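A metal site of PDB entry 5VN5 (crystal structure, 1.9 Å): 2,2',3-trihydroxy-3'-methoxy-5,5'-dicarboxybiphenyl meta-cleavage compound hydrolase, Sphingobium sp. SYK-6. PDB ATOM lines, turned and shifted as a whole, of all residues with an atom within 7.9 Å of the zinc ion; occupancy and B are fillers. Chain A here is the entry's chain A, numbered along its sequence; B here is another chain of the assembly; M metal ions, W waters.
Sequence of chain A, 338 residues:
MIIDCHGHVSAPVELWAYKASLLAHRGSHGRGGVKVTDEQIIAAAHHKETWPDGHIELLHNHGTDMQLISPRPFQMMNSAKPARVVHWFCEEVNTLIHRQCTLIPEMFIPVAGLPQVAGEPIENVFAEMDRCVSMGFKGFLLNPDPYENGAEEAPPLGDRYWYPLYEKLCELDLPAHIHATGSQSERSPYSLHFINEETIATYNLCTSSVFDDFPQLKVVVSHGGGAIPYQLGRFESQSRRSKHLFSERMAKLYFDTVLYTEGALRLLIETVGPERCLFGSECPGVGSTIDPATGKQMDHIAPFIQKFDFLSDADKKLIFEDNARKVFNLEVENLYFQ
The side-chain hydroxyl of Ser 70 sits at hydrogen-bond distance from a ring nitrogen (ND1) of His 8 (2.9 Å).
A ring nitrogen (ND1) of His 8 is in hydrogen-bond range of the backbone carbonyl oxygen (O) of Pro 71 (3.1 Å).
A ring nitrogen (ND1) of His 6 lies within hydrogen-bond range of the side-chain carboxylate (OD2) of Asp 256, at 2.7 Å.
The side-chain carboxylate of Glu 282 is in hydrogen-bond range of a ring nitrogen (NE2) of His 223, 2.7 Å away.
The side-chain carboxylate (OE1) of Glu 282 lies within salt-bridge range of the guanidinium group (NH1) of Arg 234 of chain B, 3.4 Å away.
The nearest printed residue that does not touch the zinc ion is His 223 (4.3 Å).
The zinc ion is bound by a ring nitrogen (NE2) of His 179 (2.1 Å), a ring nitrogen (NE2) of His 8 (2.1 Å), a ring nitrogen (NE2) of His 6 (2.1 Å), the side-chain carboxylate (OE2) of Glu 282 (2.2 Å) and water W1 (2.5 Å).
The zinc ion has five donor atoms within binding distance.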
ATOM      1  N   HIS A   6     -30.046 -13.653   4.613  1.00  0.00           N
ATOM      2  CA  HIS A   6     -29.678 -14.979   4.104  1.00  0.00           C
ATOM      3  C   HIS A   6     -28.967 -15.753   5.218  1.00  0.00           C
ATOM      4  O   HIS A   6     -27.743 -15.737   5.318  1.00  0.00           O
ATOM      5  CB  HIS A   6     -28.806 -14.854   2.857  1.00  0.00           C
ATOM      6  CG  HIS A   6     -28.611 -16.126   2.086  1.00  0.00           C
ATOM      7  ND1 HIS A   6     -28.448 -16.134   0.716  1.00  0.00           N
ATOM      8  CD2 HIS A   6     -28.541 -17.424   2.476  1.00  0.00           C
ATOM      9  CE1 HIS A   6     -28.283 -17.368   0.299  1.00  0.00           C
ATOM     10  NE2 HIS A   6     -28.347 -18.182   1.344  1.00  0.00           N
ATOM     11  N   GLY A   7     -29.760 -16.423   6.054  1.00  0.00           N
ATOM     12  CA  GLY A   7     -29.226 -17.384   6.988  1.00  0.00           C
ATOM     13  C   GLY A   7     -30.011 -18.682   6.864  1.00  0.00           C
ATOM     14  O   GLY A   7     -31.108 -18.702   6.328  1.00  0.00           O
ATOM     15  N   HIS A   8     -29.427 -19.765   7.394  1.00  0.00           N
ATOM     16  CA  HIS A   8     -30.107 -21.051   7.395  1.00  0.00           C
ATOM     17  C   HIS A   8     -30.168 -21.604   8.806  1.00  0.00           C
ATOM     18  O   HIS A   8     -29.276 -21.377   9.630  1.00  0.00           O
ATOM     19  CB  HIS A   8     -29.426 -22.038   6.450  1.00  0.00           C
ATOM     20  CG  HIS A   8     -29.343 -21.540   5.042  1.00  0.00           C
ATOM     21  ND1 HIS A   8     -30.424 -21.001   4.373  1.00  0.00           N
ATOM     22  CD2 HIS A   8     -28.297 -21.452   4.183  1.00  0.00           C
ATOM     23  CE1 HIS A   8     -30.051 -20.631   3.156  1.00  0.00           C
ATOM     24  NE2 HIS A   8     -28.769 -20.890   3.027  1.00  0.00           N
ATOM     25  N   SER A  70     -33.954 -19.632   6.822  1.00  0.00           N
ATOM     26  CA  SER A  70     -34.650 -20.537   5.925  1.00  0.00           C
ATOM     27  C   SER A  70     -34.098 -21.947   6.087  1.00  0.00           C
ATOM     28  O   SER A  70     -33.130 -22.139   6.830  1.00  0.00           O
ATOM     29  CB  SER A  70     -34.492 -20.037   4.494  1.00  0.00           C
ATOM     30  OG  SER A  70     -33.109 -19.846   4.200  1.00  0.00           O
ATOM     31  N   PRO A  71     -34.713 -22.967   5.457  1.00  0.00           N
ATOM     32  CA  PRO A  71     -34.135 -24.315   5.490  1.00  0.00           C
ATOM     33  C   PRO A  71     -32.707 -24.305   4.976  1.00  0.00           C
ATOM     34  O   PRO A  71     -32.305 -23.424   4.215  1.00  0.00           O
ATOM     35  CB  PRO A  71     -35.070 -25.123   4.562  1.00  0.00           C
ATOM     36  CG  PRO A  71     -36.383 -24.408   4.643  1.00  0.00           C
ATOM     37  CD  PRO A  71     -35.985 -22.927   4.719  1.00  0.00           C
ATOM     38  N   ARG A  72     -31.923 -25.273   5.439  1.00  0.00           N
ATOM     39  CA  ARG A  72     -30.603 -25.536   4.850  1.00  0.00           C
ATOM     40  C   ARG A  72     -30.860 -26.145   3.478  1.00  0.00           C
ATOM     41  O   ARG A  72     -31.367 -27.284   3.415  1.00  0.00           O
ATOM     42  CB  ARG A  72     -29.784 -26.472   5.718  1.00  0.00           C
ATOM     43  CG  ARG A  72     -29.383 -25.849   7.039  1.00  0.00           C
ATOM     44  CD  ARG A  72     -28.405 -26.720   7.807  1.00  0.00           C
ATOM     45  NE  ARG A  72     -27.952 -26.082   9.038  1.00  0.00           N
ATOM     46  CZ  ARG A  72     -27.163 -26.667   9.933  1.00  0.00           C
ATOM     47  NH1 ARG A  72     -26.781 -25.996  11.023  1.00  0.00           N
ATOM     48  NH2 ARG A  72     -26.737 -27.920   9.747  1.00  0.00           N
ATOM     49  N   PRO A  73     -30.597 -25.437   2.369  1.00  0.00           N
ATOM     50  CA  PRO A  73     -31.095 -25.931   1.077  1.00  0.00           C
ATOM     51  C   PRO A  73     -30.512 -27.257   0.645  1.00  0.00           C
ATOM     52  O   PRO A  73     -31.237 -28.020  -0.003  1.00  0.00           O
ATOM     53  CB  PRO A  73     -30.736 -24.797   0.101  1.00  0.00           C
ATOM     54  CG  PRO A  73     -30.755 -23.554   0.990  1.00  0.00           C
ATOM     55  CD  PRO A  73     -30.120 -24.052   2.271  1.00  0.00           C
ATOM     56  N   PHE A  74     -29.240 -27.545   0.945  1.00  0.00           N
ATOM     57  CA  PHE A  74     -28.634 -28.774   0.454  1.00  0.00           C
ATOM     58  C   PHE A  74     -29.271 -30.021   1.077  1.00  0.00           C
ATOM     59  O   PHE A  74     -29.016 -31.123   0.590  1.00  0.00           O
ATOM     60  CB  PHE A  74     -27.110 -28.753   0.671  1.00  0.00           C
ATOM     61  CG  PHE A  74     -26.655 -29.149   2.047  1.00  0.00           C
ATOM     62  CD1 PHE A  74     -26.994 -28.409   3.157  1.00  0.00           C
ATOM     63  CD2 PHE A  74     -25.853 -30.242   2.229  1.00  0.00           C
ATOM     64  CE1 PHE A  74     -26.559 -28.777   4.439  1.00  0.00           C
ATOM     65  CE2 PHE A  74     -25.421 -30.608   3.497  1.00  0.00           C
ATOM     66  CZ  PHE A  74     -25.770 -29.861   4.596  1.00  0.00           C
ATOM     67  N   LEU A 141     -37.937 -19.723  -0.285  1.00  0.00           N
ATOM     68  CA  LEU A 141     -36.832 -20.173  -1.127  1.00  0.00           C
ATOM     69  C   LEU A 141     -37.381 -20.853  -2.378  1.00  0.00           C
ATOM     70  O   LEU A 141     -38.184 -21.791  -2.294  1.00  0.00           O
ATOM     71  CB  LEU A 141     -35.917 -21.152  -0.394  1.00  0.00           C
ATOM     72  CG  LEU A 141     -35.205 -20.671   0.878  1.00  0.00           C
ATOM     73  CD1 LEU A 141     -34.121 -21.665   1.251  1.00  0.00           C
ATOM     74  CD2 LEU A 141     -34.599 -19.267   0.755  1.00  0.00           C
ATOM     75  N   HIS A 177     -36.836 -16.235  -2.991  1.00  0.00           N
ATOM     76  CA  HIS A 177     -35.400 -16.129  -2.767  1.00  0.00           C
ATOM     77  C   HIS A 177     -34.748 -17.284  -3.521  1.00  0.00           C
ATOM     78  O   HIS A 177     -34.824 -18.440  -3.083  1.00  0.00           O
ATOM     79  CB  HIS A 177     -35.109 -16.160  -1.267  1.00  0.00           C
ATOM     80  CG  HIS A 177     -33.787 -15.609  -0.899  1.00  0.00           C
ATOM     81  ND1 HIS A 177     -33.468 -15.279   0.398  1.00  0.00           N
ATOM     82  CD2 HIS A 177     -32.681 -15.353  -1.641  1.00  0.00           C
ATOM     83  CE1 HIS A 177     -32.231 -14.797   0.434  1.00  0.00           C
ATOM     84  NE2 HIS A 177     -31.736 -14.835  -0.794  1.00  0.00           N
ATOM     85  N   ILE A 178     -34.131 -16.976  -4.661  1.00  0.00           N
ATOM     86  CA  ILE A 178     -33.599 -18.027  -5.515  1.00  0.00           C
ATOM     87  C   ILE A 178     -32.493 -18.758  -4.766  1.00  0.00           C
ATOM     88  O   ILE A 178     -31.509 -18.133  -4.337  1.00  0.00           O
ATOM     89  CB  ILE A 178     -33.036 -17.463  -6.831  1.00  0.00           C
ATOM     90  CG1 ILE A 178     -34.068 -16.657  -7.595  1.00  0.00           C
ATOM     91  CG2 ILE A 178     -32.452 -18.559  -7.702  1.00  0.00           C
ATOM     92  CD1 ILE A 178     -35.276 -17.420  -8.057  1.00  0.00           C
ATOM     93  N   HIS A 179     -32.628 -20.078  -4.662  1.00  0.00           N
ATOM     94  CA  HIS A 179     -31.631 -20.907  -3.988  1.00  0.00           C
ATOM     95  C   HIS A 179     -31.797 -22.329  -4.472  1.00  0.00           C
ATOM     96  O   HIS A 179     -32.871 -22.924  -4.288  1.00  0.00           O
ATOM     97  CB  HIS A 179     -31.803 -20.853  -2.472  1.00  0.00           C
ATOM     98  CG  HIS A 179     -30.518 -20.995  -1.720  1.00  0.00           C
ATOM     99  ND1 HIS A 179     -29.671 -22.064  -1.887  1.00  0.00           N
ATOM    100  CD2 HIS A 179     -29.973 -20.229  -0.755  1.00  0.00           C
ATOM    101  CE1 HIS A 179     -28.626 -21.919  -1.084  1.00  0.00           C
ATOM    102  NE2 HIS A 179     -28.796 -20.812  -0.390  1.00  0.00           N
ATOM    103  N   ALA A 180     -30.751 -22.883  -5.095  1.00  0.00           N
ATOM    104  CA  ALA A 180     -30.751 -24.262  -5.472  1.00  0.00           C
ATOM    105  C   ALA A 180     -30.551 -25.117  -4.212  1.00  0.00           C
ATOM    106  O   ALA A 180     -30.227 -24.610  -3.121  1.00  0.00           O
ATOM    107  CB  ALA A 180     -29.658 -24.540  -6.516  1.00  0.00           C
ATOM    108  N   PHE A 194     -24.906 -24.187  -6.540  1.00  0.00           N
ATOM    109  CA  PHE A 194     -25.657 -22.988  -6.123  1.00  0.00           C
ATOM    110  C   PHE A 194     -25.429 -21.847  -7.106  1.00  0.00           C
ATOM    111  O   PHE A 194     -26.372 -21.179  -7.564  1.00  0.00           O
ATOM    112  CB  PHE A 194     -25.232 -22.463  -4.724  1.00  0.00           C
ATOM    113  CG  PHE A 194     -25.660 -23.314  -3.531  1.00  0.00           C
ATOM    114  CD1 PHE A 194     -26.697 -24.216  -3.639  1.00  0.00           C
ATOM    115  CD2 PHE A 194     -25.024 -23.161  -2.296  1.00  0.00           C
ATOM    116  CE1 PHE A 194     -27.095 -24.979  -2.551  1.00  0.00           C
ATOM    117  CE2 PHE A 194     -25.424 -23.901  -1.190  1.00  0.00           C
ATOM    118  CZ  PHE A 194     -26.472 -24.844  -1.352  1.00  0.00           C
ATOM    119  N   GLU A 198     -27.944 -20.038  -9.765  1.00  0.00           N
ATOM    120  CA  GLU A 198     -28.272 -18.615  -9.683  1.00  0.00           C
ATOM    121  C   GLU A 198     -28.054 -17.939 -11.019  1.00  0.00           C
ATOM    122  O   GLU A 198     -28.836 -17.080 -11.438  1.00  0.00           O
ATOM    123  CB  GLU A 198     -27.420 -17.941  -8.615  1.00  0.00           C
ATOM    124  CG  GLU A 198     -27.832 -18.359  -7.220  1.00  0.00           C
ATOM    125  CD  GLU A 198     -26.689 -18.358  -6.237  1.00  0.00           C
ATOM    126  OE1 GLU A 198     -25.570 -17.932  -6.590  1.00  0.00           O
ATOM    127  OE2 GLU A 198     -26.929 -18.826  -5.105  1.00  0.00           O
ATOM    128  N   SER A 222     -29.722 -15.224  -4.755  1.00  0.00           N
ATOM    129  CA  SER A 222     -28.681 -15.498  -3.776  1.00  0.00           C
ATOM    130  C   SER A 222     -27.277 -15.277  -4.340  1.00  0.00           C
ATOM    131  O   SER A 222     -27.025 -15.340  -5.539  1.00  0.00           O
ATOM    132  CB  SER A 222     -28.785 -16.920  -3.261  1.00  0.00           C
ATOM    133  OG  SER A 222     -29.943 -17.066  -2.473  1.00  0.00           O
ATOM    134  N   HIS A 223     -26.337 -15.064  -3.412  1.00  0.00           N
ATOM    135  CA  HIS A 223     -24.903 -15.018  -3.711  1.00  0.00           C
ATOM    136  C   HIS A 223     -24.563 -13.994  -4.792  1.00  0.00           C
ATOM    137  O   HIS A 223     -23.807 -14.278  -5.734  1.00  0.00           O
ATOM    138  CB  HIS A 223     -24.386 -16.405  -4.100  1.00  0.00           C
ATOM    139  CG  HIS A 223     -24.613 -17.451  -3.032  1.00  0.00           C
ATOM    140  ND1 HIS A 223     -25.483 -18.504  -3.188  1.00  0.00           N
ATOM    141  CD2 HIS A 223     -24.089 -17.572  -1.791  1.00  0.00           C
ATOM    142  CE1 HIS A 223     -25.479 -19.243  -2.090  1.00  0.00           C
ATOM    143  NE2 HIS A 223     -24.641 -18.699  -1.223  1.00  0.00           N
ATOM    144  N   ASP A 256     -28.859 -10.558  -2.983  1.00  0.00           N
ATOM    145  CA  ASP A 256     -28.272 -10.485  -1.645  1.00  0.00           C
ATOM    146  C   ASP A 256     -26.739 -10.354  -1.774  1.00  0.00           C
ATOM    147  O   ASP A 256     -26.158 -10.538  -2.855  1.00  0.00           O
ATOM    148  CB  ASP A 256     -28.725 -11.666  -0.748  1.00  0.00           C
ATOM    149  CG  ASP A 256     -28.094 -13.007  -1.076  1.00  0.00           C
ATOM    150  OD1 ASP A 256     -26.923 -13.096  -1.451  1.00  0.00           O
ATOM    151  OD2 ASP A 256     -28.801 -14.019  -0.876  1.00  0.00           O
ATOM    152  N   VAL A 258     -24.203 -12.129  -0.369  1.00  0.00           N
ATOM    153  CA  VAL A 258     -23.431 -13.241   0.146  1.00  0.00           C
ATOM    154  C   VAL A 258     -22.246 -13.468  -0.788  1.00  0.00           C
ATOM    155  O   VAL A 258     -22.269 -14.334  -1.675  1.00  0.00           O
ATOM    156  CB  VAL A 258     -24.263 -14.518   0.327  1.00  0.00           C
ATOM    157  CG1 VAL A 258     -23.367 -15.598   0.934  1.00  0.00           C
ATOM    158  CG2 VAL A 258     -25.470 -14.240   1.184  1.00  0.00           C
ATOM    159  N   TYR A 260     -17.798 -13.062  -0.339  1.00  0.00           N
ATOM    160  CA  TYR A 260     -16.812 -12.962   0.733  1.00  0.00           C
ATOM    161  C   TYR A 260     -15.505 -12.301   0.302  1.00  0.00           C
ATOM    162  O   TYR A 260     -14.485 -12.446   0.995  1.00  0.00           O
ATOM    163  CB  TYR A 260     -16.549 -14.355   1.303  1.00  0.00           C
ATOM    164  CG  TYR A 260     -17.793 -15.054   1.825  1.00  0.00           C
ATOM    165  CD1 TYR A 260     -18.732 -14.379   2.585  1.00  0.00           C
ATOM    166  CD2 TYR A 260     -18.032 -16.395   1.534  1.00  0.00           C
ATOM    167  CE1 TYR A 260     -19.870 -15.022   3.076  1.00  0.00           C
ATOM    168  CE2 TYR A 260     -19.174 -17.054   2.009  1.00  0.00           C
ATOM    169  CZ  TYR A 260     -20.086 -16.353   2.788  1.00  0.00           C
ATOM    170  OH  TYR A 260     -21.209 -17.001   3.254  1.00  0.00           O
ATOM    171  N   SER A 281     -25.355 -12.841   4.613  1.00  0.00           N
ATOM    172  CA  SER A 281     -24.027 -13.389   4.892  1.00  0.00           C
ATOM    173  C   SER A 281     -23.905 -14.912   4.901  1.00  0.00           C
ATOM    174  O   SER A 281     -22.776 -15.409   4.807  1.00  0.00           O
ATOM    175  CB  SER A 281     -23.527 -12.902   6.248  1.00  0.00           C
ATOM    176  OG  SER A 281     -24.144 -13.640   7.307  1.00  0.00           O
ATOM    177  N   GLU A 282     -24.998 -15.669   5.034  1.00  0.00           N
ATOM    178  CA  GLU A 282     -24.944 -17.127   5.167  1.00  0.00           C
ATOM    179  C   GLU A 282     -24.191 -17.548   6.439  1.00  0.00           C
ATOM    180  O   GLU A 282     -23.774 -18.720   6.557  1.00  0.00           O
ATOM    181  CB  GLU A 282     -24.332 -17.791   3.905  1.00  0.00           C
ATOM    182  CG  GLU A 282     -25.371 -18.610   3.020  1.00  0.00           C
ATOM    183  CD  GLU A 282     -24.834 -19.351   1.728  1.00  0.00           C
ATOM    184  OE1 GLU A 282     -23.683 -19.051   1.265  1.00  0.00           O
ATOM    185  OE2 GLU A 282     -25.595 -20.236   1.168  1.00  0.00           O
ATOM    186  N   VAL A 286     -20.682 -21.679   5.003  1.00  0.00           N
ATOM    187  CA  VAL A 286     -19.550 -21.887   4.104  1.00  0.00           C
ATOM    188  C   VAL A 286     -18.428 -20.896   4.409  1.00  0.00           C
ATOM    189  O   VAL A 286     -17.239 -21.221   4.337  1.00  0.00           O
ATOM    190  CB  VAL A 286     -20.043 -21.759   2.646  1.00  0.00           C
ATOM    191  CG1 VAL A 286     -18.922 -21.972   1.684  1.00  0.00           C
ATOM    192  CG2 VAL A 286     -21.179 -22.756   2.358  1.00  0.00           C
ATOM    193  N   ARG B 234     -16.095 -17.616  -1.418  1.00  0.00           N
ATOM    194  CA  ARG B 234     -16.756 -18.811  -0.886  1.00  0.00           C
ATOM    195  C   ARG B 234     -15.970 -20.077  -1.180  1.00  0.00           C
ATOM    196  O   ARG B 234     -15.932 -20.998  -0.337  1.00  0.00           O
ATOM    197  CB  ARG B 234     -18.187 -18.949  -1.428  1.00  0.00           C
ATOM    198  CG  ARG B 234     -18.292 -19.431  -2.877  1.00  0.00           C
ATOM    199  CD  ARG B 234     -19.744 -19.487  -3.413  1.00  0.00           C
ATOM    200  NE  ARG B 234     -20.541 -20.473  -2.673  1.00  0.00           N
ATOM    201  CZ  ARG B 234     -21.224 -20.201  -1.558  1.00  0.00           C
ATOM    202  NH1 ARG B 234     -21.240 -18.957  -1.041  1.00  0.00           N
ATOM    203  NH2 ARG B 234     -21.882 -21.182  -0.950  1.00  0.00           N
HETATM  204 ZN    ZN M   1     -27.814 -20.243   1.323  1.00  0.00          ZN
HETATM  205  O   HOH W   1     -26.802 -22.492   1.481  1.00  0.00           O
